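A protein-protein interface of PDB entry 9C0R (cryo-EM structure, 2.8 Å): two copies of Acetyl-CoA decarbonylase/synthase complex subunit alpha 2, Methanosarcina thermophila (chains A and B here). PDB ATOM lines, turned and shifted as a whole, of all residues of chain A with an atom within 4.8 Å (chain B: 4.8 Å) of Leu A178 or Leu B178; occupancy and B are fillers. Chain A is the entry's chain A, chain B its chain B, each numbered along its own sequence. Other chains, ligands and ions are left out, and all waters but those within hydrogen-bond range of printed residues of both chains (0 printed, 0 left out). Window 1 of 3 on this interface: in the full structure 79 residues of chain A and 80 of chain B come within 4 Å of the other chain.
The side-chain hydroxyl (OG1) of Thr B111 sits at hydrogen-bond distance from the backbone carbonyl oxygen (O) of Leu B107 (2.7 Å).
OG1 of Thr A111 sits at hydrogen-bond distance from O of Leu A107, 2.7 Å away.
Among the printed residues, merely in contact across the chains: Ala A179 with Ala B114, Ala A114 with Ala B179, Leu A174 with Leu B178, Leu A178 with Leu B174, Ala A114 with Leu B178, Leu A178 with Ala B114, Thr A111 with His B182, His A182 with Thr B111, Leu A178 with Leu B178, Leu A107 with Leu B107, Ile A110 with Leu B178, Leu A178 with Ile B110, Ala A114 with Gly B175 and Gly A175 with Ala B114.
Of chain B, only Ile B110 (3.97 Å), Ala B114 (3.6 Å), Leu B174 (3.6 Å) and Leu B178 (3.8 Å) come within 4 Å of Leu A178.
Leu B178 touches just these residues of chain A: Ile A110 (3.96 Å), Ala A114 (3.6 Å), Leu A174 (3.6 Å) and Leu A178 (3.8 Å).
Of the printed residues of chain A, Gly B175 touches Ala A114 (3.99 Å).
Printed residues of chain B within 4 Å of Ala A114: Gly B175 (3.99 Å), Leu B178 (3.6 Å) and Ala B179 (3.3 Å).
Of the printed residues of chain A, His B182 touches Thr A111.
Printed residues of chain B within 4 Å of Leu A107: Leu B107.
Of the printed residues of chain B, Leu A174 touches Leu B178 (3.6 Å).
Of the 13 printed residues of chain A, 9 touch a printed residue of chain B.
Hydrophobic or aromatic side chains of chain A within 4 Å of the printed part of chain B: Leu A107, Ala A114, Leu A174, Leu A178 and Ala A179.
Of the 13 printed residues of chain B, 9 touch a printed residue of chain A.
Printed residues of chain B that touch a printed residue of chain A: Leu B107, Ile B110, Thr B111, Ala B114, Leu B174, Gly B175, Leu B178, Ala B179 and His B182.
Hydrophobic or aromatic side chains of chain B that line the printed part of chain A: Leu B107, Ala B114, Leu B174, Leu B178 and Ala B179.
Among the printed residues, 14 pairs touch across the chains.
Ala A114 touches Gly B175, and with the chains exchanged Gly A175 touches Ala B114.
Ala A114 touches Leu B178, and with the chains exchanged Leu A178 touches Ala B114.
Ala A114 touches Ala B179, and with the chains exchanged Ala A179 touches Ala B114.
Leu A174 touches Leu B178, and with the chains exchanged Leu A178 touches Leu B174.
Positions printed for both chains: 107, 110, 111, 114, 174, 175, 176, 177, 178, 179, 180, 181 and 182.
Of the 14 pairs that touch across the chains among the printed residues, 14 have their exchanged pair printed and touching as well.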
ATOM      1  N   LEU A 107      11.845 -14.930 -16.623  1.00  0.00           N
ATOM      2  CA  LEU A 107      11.448 -13.814 -15.771  1.00  0.00           C
ATOM      3  C   LEU A 107      10.991 -12.621 -16.602  1.00  0.00           C
ATOM      4  O   LEU A 107      10.000 -11.964 -16.265  1.00  0.00           O
ATOM      5  CB  LEU A 107      12.604 -13.420 -14.853  1.00  0.00           C
ATOM      6  CG  LEU A 107      12.375 -12.248 -13.896  1.00  0.00           C
ATOM      7  CD1 LEU A 107      11.144 -12.470 -13.031  1.00  0.00           C
ATOM      8  CD2 LEU A 107      13.602 -12.024 -13.033  1.00  0.00           C
ATOM      9  N   ILE A 110       7.458 -13.477 -17.948  1.00  0.00           N
ATOM     10  CA  ILE A 110       6.400 -13.396 -16.947  1.00  0.00           C
ATOM     11  C   ILE A 110       6.176 -11.954 -16.514  1.00  0.00           C
ATOM     12  O   ILE A 110       5.053 -11.579 -16.173  1.00  0.00           O
ATOM     13  CB  ILE A 110       6.677 -14.312 -15.739  1.00  0.00           C
ATOM     14  CG1 ILE A 110       7.931 -13.881 -14.985  1.00  0.00           C
ATOM     15  CG2 ILE A 110       6.778 -15.756 -16.177  1.00  0.00           C
ATOM     16  CD1 ILE A 110       8.190 -14.698 -13.751  1.00  0.00           C
ATOM     17  N   THR A 111       7.219 -11.119 -16.524  1.00  0.00           N
ATOM     18  CA  THR A 111       7.022  -9.704 -16.220  1.00  0.00           C
ATOM     19  C   THR A 111       6.123  -9.041 -17.258  1.00  0.00           C
ATOM     20  O   THR A 111       5.196  -8.297 -16.911  1.00  0.00           O
ATOM     21  CB  THR A 111       8.373  -8.991 -16.142  1.00  0.00           C
ATOM     22  OG1 THR A 111       9.211  -9.657 -15.190  1.00  0.00           O
ATOM     23  CG2 THR A 111       8.189  -7.550 -15.715  1.00  0.00           C
ATOM     24  N   ALA A 114       2.655 -10.144 -16.725  1.00  0.00           N
ATOM     25  CA  ALA A 114       2.084  -9.496 -15.553  1.00  0.00           C
ATOM     26  C   ALA A 114       1.619  -8.086 -15.873  1.00  0.00           C
ATOM     27  O   ALA A 114       0.563  -7.655 -15.404  1.00  0.00           O
ATOM     28  CB  ALA A 114       3.099  -9.476 -14.413  1.00  0.00           C
ATOM     29  N   LEU A 174       0.074 -16.999 -13.195  1.00  0.00           N
ATOM     30  CA  LEU A 174       1.162 -16.054 -12.983  1.00  0.00           C
ATOM     31  C   LEU A 174       1.811 -16.266 -11.623  1.00  0.00           C
ATOM     32  O   LEU A 174       3.038 -16.192 -11.495  1.00  0.00           O
ATOM     33  CB  LEU A 174       0.633 -14.627 -13.108  1.00  0.00           C
ATOM     34  CG  LEU A 174       1.225 -13.760 -14.214  1.00  0.00           C
ATOM     35  CD1 LEU A 174       0.617 -12.379 -14.144  1.00  0.00           C
ATOM     36  CD2 LEU A 174       2.735 -13.693 -14.098  1.00  0.00           C
ATOM     37  N   GLY A 175       1.000 -16.523 -10.596  1.00  0.00           N
ATOM     38  CA  GLY A 175       1.556 -16.803  -9.283  1.00  0.00           C
ATOM     39  C   GLY A 175       2.438 -18.035  -9.284  1.00  0.00           C
ATOM     40  O   GLY A 175       3.543 -18.025  -8.733  1.00  0.00           O
ATOM     41  N   GLN A 176       1.968 -19.111  -9.922  1.00  0.00           N
ATOM     42  CA  GLN A 176       2.780 -20.327 -10.004  1.00  0.00           C
ATOM     43  C   GLN A 176       4.088 -20.075 -10.754  1.00  0.00           C
ATOM     44  O   GLN A 176       5.171 -20.490 -10.311  1.00  0.00           O
ATOM     45  CB  GLN A 176       1.986 -21.448 -10.675  1.00  0.00           C
ATOM     46  CG  GLN A 176       0.605 -21.682 -10.091  1.00  0.00           C
ATOM     47  CD  GLN A 176       0.643 -22.404  -8.759  1.00  0.00           C
ATOM     48  OE1 GLN A 176       1.293 -23.439  -8.620  1.00  0.00           O
ATOM     49  NE2 GLN A 176      -0.059 -21.863  -7.773  1.00  0.00           N
ATOM     50  N   LEU A 177       4.008 -19.381 -11.892  1.00  0.00           N
ATOM     51  CA  LEU A 177       5.204 -19.151 -12.695  1.00  0.00           C
ATOM     52  C   LEU A 177       6.204 -18.260 -11.970  1.00  0.00           C
ATOM     53  O   LEU A 177       7.416 -18.478 -12.067  1.00  0.00           O
ATOM     54  CB  LEU A 177       4.822 -18.551 -14.046  1.00  0.00           C
ATOM     55  CG  LEU A 177       4.003 -19.462 -14.961  1.00  0.00           C
ATOM     56  CD1 LEU A 177       3.773 -18.804 -16.307  1.00  0.00           C
ATOM     57  CD2 LEU A 177       4.686 -20.809 -15.125  1.00  0.00           C
ATOM     58  N   LEU A 178       5.722 -17.250 -11.244  1.00  0.00           N
ATOM     59  CA  LEU A 178       6.631 -16.402 -10.481  1.00  0.00           C
ATOM     60  C   LEU A 178       7.239 -17.164  -9.313  1.00  0.00           C
ATOM     61  O   LEU A 178       8.398 -16.933  -8.949  1.00  0.00           O
ATOM     62  CB  LEU A 178       5.907 -15.149  -9.993  1.00  0.00           C
ATOM     63  CG  LEU A 178       6.742 -14.184  -9.148  1.00  0.00           C
ATOM     64  CD1 LEU A 178       7.939 -13.657  -9.928  1.00  0.00           C
ATOM     65  CD2 LEU A 178       5.885 -13.040  -8.643  1.00  0.00           C
ATOM     66  N   ALA A 179       6.472 -18.075  -8.705  1.00  0.00           N
ATOM     67  CA  ALA A 179       7.037 -18.936  -7.675  1.00  0.00           C
ATOM     68  C   ALA A 179       8.171 -19.784  -8.226  1.00  0.00           C
ATOM     69  O   ALA A 179       9.140 -20.065  -7.513  1.00  0.00           O
ATOM     70  CB  ALA A 179       5.952 -19.830  -7.084  1.00  0.00           C
ATOM     71  N   THR A 180       8.068 -20.196  -9.488  1.00  0.00           N
ATOM     72  CA  THR A 180       9.138 -20.980 -10.099  1.00  0.00           C
ATOM     73  C   THR A 180      10.452 -20.209 -10.245  1.00  0.00           C
ATOM     74  O   THR A 180      11.490 -20.832 -10.486  1.00  0.00           O
ATOM     75  CB  THR A 180       8.685 -21.501 -11.465  1.00  0.00           C
ATOM     76  OG1 THR A 180       7.309 -21.893 -11.389  1.00  0.00           O
ATOM     77  CG2 THR A 180       9.507 -22.703 -11.876  1.00  0.00           C
ATOM     78  N   VAL A 181      10.441 -18.881 -10.095  1.00  0.00           N
ATOM     79  CA  VAL A 181      11.658 -18.084 -10.252  1.00  0.00           C
ATOM     80  C   VAL A 181      12.619 -18.258  -9.075  1.00  0.00           C
ATOM     81  O   VAL A 181      13.825 -18.022  -9.222  1.00  0.00           O
ATOM     82  CB  VAL A 181      11.258 -16.607 -10.469  1.00  0.00           C
ATOM     83  CG1 VAL A 181      12.403 -15.645 -10.175  1.00  0.00           C
ATOM     84  CG2 VAL A 181      10.761 -16.406 -11.886  1.00  0.00           C
ATOM     85  N   HIS A 182      12.119 -18.711  -7.924  1.00  0.00           N
ATOM     86  CA  HIS A 182      12.923 -18.846  -6.713  1.00  0.00           C
ATOM     87  C   HIS A 182      14.172 -19.683  -6.955  1.00  0.00           C
ATOM     88  O   HIS A 182      14.233 -20.502  -7.875  1.00  0.00           O
ATOM     89  CB  HIS A 182      12.085 -19.496  -5.615  1.00  0.00           C
ATOM     90  CG  HIS A 182      12.653 -19.359  -4.237  1.00  0.00           C
ATOM     91  ND1 HIS A 182      13.467 -20.314  -3.669  1.00  0.00           N
ATOM     92  CD2 HIS A 182      12.493 -18.396  -3.299  1.00  0.00           C
ATOM     93  CE1 HIS A 182      13.801 -19.936  -2.448  1.00  0.00           C
ATOM     94  NE2 HIS A 182      13.223 -18.776  -2.200  1.00  0.00           N
ATOM     95  N   LEU B 107      11.762  -7.258  -6.010  1.00  0.00           N
ATOM     96  CA  LEU B 107      11.620  -8.485  -6.785  1.00  0.00           C
ATOM     97  C   LEU B 107      11.902  -9.715  -5.930  1.00  0.00           C
ATOM     98  O   LEU B 107      11.193 -10.722  -6.026  1.00  0.00           O
ATOM     99  CB  LEU B 107      12.549  -8.449  -7.997  1.00  0.00           C
ATOM    100  CG  LEU B 107      12.550  -9.670  -8.919  1.00  0.00           C
ATOM    101  CD1 LEU B 107      11.148  -9.992  -9.415  1.00  0.00           C
ATOM    102  CD2 LEU B 107      13.492  -9.450 -10.087  1.00  0.00           C
ATOM    103  N   ILE B 110       8.810 -10.227  -3.649  1.00  0.00           N
ATOM    104  CA  ILE B 110       7.641 -10.768  -4.335  1.00  0.00           C
ATOM    105  C   ILE B 110       7.890 -12.204  -4.773  1.00  0.00           C
ATOM    106  O   ILE B 110       6.953 -13.005  -4.822  1.00  0.00           O
ATOM    107  CB  ILE B 110       7.209  -9.884  -5.521  1.00  0.00           C
ATOM    108  CG1 ILE B 110       8.283  -9.833  -6.603  1.00  0.00           C
ATOM    109  CG2 ILE B 110       6.852  -8.493  -5.048  1.00  0.00           C
ATOM    110  CD1 ILE B 110       7.867  -9.047  -7.814  1.00  0.00           C
ATOM    111  N   THR B 111       9.136 -12.567  -5.085  1.00  0.00           N
ATOM    112  CA  THR B 111       9.433 -13.960  -5.404  1.00  0.00           C
ATOM    113  C   THR B 111       9.171 -14.864  -4.203  1.00  0.00           C
ATOM    114  O   THR B 111       8.548 -15.925  -4.332  1.00  0.00           O
ATOM    115  CB  THR B 111      10.881 -14.094  -5.875  1.00  0.00           C
ATOM    116  OG1 THR B 111      11.110 -13.209  -6.977  1.00  0.00           O
ATOM    117  CG2 THR B 111      11.168 -15.515  -6.315  1.00  0.00           C
ATOM    118  N   ALA B 114       5.543 -15.227  -3.730  1.00  0.00           N
ATOM    119  CA  ALA B 114       4.979 -16.110  -4.742  1.00  0.00           C
ATOM    120  C   ALA B 114       5.202 -17.570  -4.388  1.00  0.00           C
ATOM    121  O   ALA B 114       4.314 -18.402  -4.583  1.00  0.00           O
ATOM    122  CB  ALA B 114       5.579 -15.795  -6.110  1.00  0.00           C
ATOM    123  N   LEU B 174      -0.337 -10.120  -6.069  1.00  0.00           N
ATOM    124  CA  LEU B 174       0.934 -10.578  -6.613  1.00  0.00           C
ATOM    125  C   LEU B 174       1.064 -10.206  -8.083  1.00  0.00           C
ATOM    126  O   LEU B 174       2.142  -9.804  -8.535  1.00  0.00           O
ATOM    127  CB  LEU B 174       1.056 -12.089  -6.430  1.00  0.00           C
ATOM    128  CG  LEU B 174       2.209 -12.594  -5.570  1.00  0.00           C
ATOM    129  CD1 LEU B 174       2.192 -14.105  -5.550  1.00  0.00           C
ATOM    130  CD2 LEU B 174       3.536 -12.074  -6.085  1.00  0.00           C
ATOM    131  N   GLY B 175      -0.023 -10.341  -8.843  1.00  0.00           N
ATOM    132  CA  GLY B 175       0.011  -9.939 -10.239  1.00  0.00           C
ATOM    133  C   GLY B 175       0.309  -8.462 -10.404  1.00  0.00           C
ATOM    134  O   GLY B 175       1.140  -8.072 -11.229  1.00  0.00           O
ATOM    135  N   GLN B 176      -0.355  -7.621  -9.605  1.00  0.00           N
ATOM    136  CA  GLN B 176      -0.091  -6.184  -9.674  1.00  0.00           C
ATOM    137  C   GLN B 176       1.360  -5.865  -9.314  1.00  0.00           C
ATOM    138  O   GLN B 176       2.036  -5.085 -10.005  1.00  0.00           O
ATOM    139  CB  GLN B 176      -1.048  -5.426  -8.754  1.00  0.00           C
ATOM    140  CG  GLN B 176      -2.513  -5.779  -8.935  1.00  0.00           C
ATOM    141  CD  GLN B 176      -3.114  -5.170 -10.186  1.00  0.00           C
ATOM    142  OE1 GLN B 176      -2.984  -3.972 -10.432  1.00  0.00           O
ATOM    143  NE2 GLN B 176      -3.779  -5.995 -10.985  1.00  0.00           N
ATOM    144  N   LEU B 177       1.864  -6.472  -8.238  1.00  0.00           N
ATOM    145  CA  LEU B 177       3.222  -6.174  -7.795  1.00  0.00           C
ATOM    146  C   LEU B 177       4.257  -6.645  -8.808  1.00  0.00           C
ATOM    147  O   LEU B 177       5.269  -5.970  -9.025  1.00  0.00           O
ATOM    148  CB  LEU B 177       3.479  -6.801  -6.427  1.00  0.00           C
ATOM    149  CG  LEU B 177       2.643  -6.231  -5.281  1.00  0.00           C
ATOM    150  CD1 LEU B 177       3.054  -6.850  -3.958  1.00  0.00           C
ATOM    151  CD2 LEU B 177       2.764  -4.719  -5.231  1.00  0.00           C
ATOM    152  N   LEU B 178       4.030  -7.801  -9.436  1.00  0.00           N
ATOM    153  CA  LEU B 178       4.960  -8.268 -10.458  1.00  0.00           C
ATOM    154  C   LEU B 178       4.889  -7.396 -11.702  1.00  0.00           C
ATOM    155  O   LEU B 178       5.904  -7.179 -12.373  1.00  0.00           O
ATOM    156  CB  LEU B 178       4.678  -9.730 -10.805  1.00  0.00           C
ATOM    157  CG  LEU B 178       5.563 -10.340 -11.894  1.00  0.00           C
ATOM    158  CD1 LEU B 178       7.032 -10.318 -11.491  1.00  0.00           C
ATOM    159  CD2 LEU B 178       5.116 -11.752 -12.214  1.00  0.00           C
ATOM    160  N   ALA B 179       3.697  -6.888 -12.032  1.00  0.00           N
ATOM    161  CA  ALA B 179       3.587  -5.933 -13.126  1.00  0.00           C
ATOM    162  C   ALA B 179       4.405  -4.682 -12.850  1.00  0.00           C
ATOM    163  O   ALA B 179       4.966  -4.089 -13.778  1.00  0.00           O
ATOM    164  CB  ALA B 179       2.126  -5.563 -13.356  1.00  0.00           C
ATOM    165  N   THR B 180       4.485  -4.271 -11.586  1.00  0.00           N
ATOM    166  CA  THR B 180       5.290  -3.103 -11.235  1.00  0.00           C
ATOM    167  C   THR B 180       6.785  -3.294 -11.495  1.00  0.00           C
ATOM    168  O   THR B 180       7.521  -2.303 -11.521  1.00  0.00           O
ATOM    169  CB  THR B 180       5.059  -2.734  -9.769  1.00  0.00           C
ATOM    170  OG1 THR B 180       3.673  -2.909  -9.449  1.00  0.00           O
ATOM    171  CG2 THR B 180       5.434  -1.288  -9.520  1.00  0.00           C
ATOM    172  N   VAL B 181       7.254  -4.528 -11.700  1.00  0.00           N
ATOM    173  CA  VAL B 181       8.679  -4.780 -11.919  1.00  0.00           C
ATOM    174  C   VAL B 181       9.144  -4.312 -13.298  1.00  0.00           C
ATOM    175  O   VAL B 181      10.338  -4.052 -13.492  1.00  0.00           O
ATOM    176  CB  VAL B 181       8.958  -6.281 -11.685  1.00  0.00           C
ATOM    177  CG1 VAL B 181      10.265  -6.736 -12.323  1.00  0.00           C
ATOM    178  CG2 VAL B 181       8.972  -6.582 -10.201  1.00  0.00           C
ATOM    179  N   HIS B 182       8.220  -4.153 -14.248  1.00  0.00           N
ATOM    180  CA  HIS B 182       8.554  -3.784 -15.620  1.00  0.00           C
ATOM    181  C   HIS B 182       9.393  -2.514 -15.674  1.00  0.00           C
ATOM    182  O   HIS B 182       9.373  -1.687 -14.758  1.00  0.00           O
ATOM    183  CB  HIS B 182       7.270  -3.572 -16.416  1.00  0.00           C
ATOM    184  CG  HIS B 182       7.458  -3.554 -17.902  1.00  0.00           C
ATOM    185  ND1 HIS B 182       7.649  -2.391 -18.615  1.00  0.00           N
ATOM    186  CD2 HIS B 182       7.442  -4.554 -18.815  1.00  0.00           C
ATOM    187  CE1 HIS B 182       7.766  -2.676 -19.899  1.00  0.00           C
ATOM    188  NE2 HIS B 182       7.645  -3.982 -20.047  1.00  0.00           N
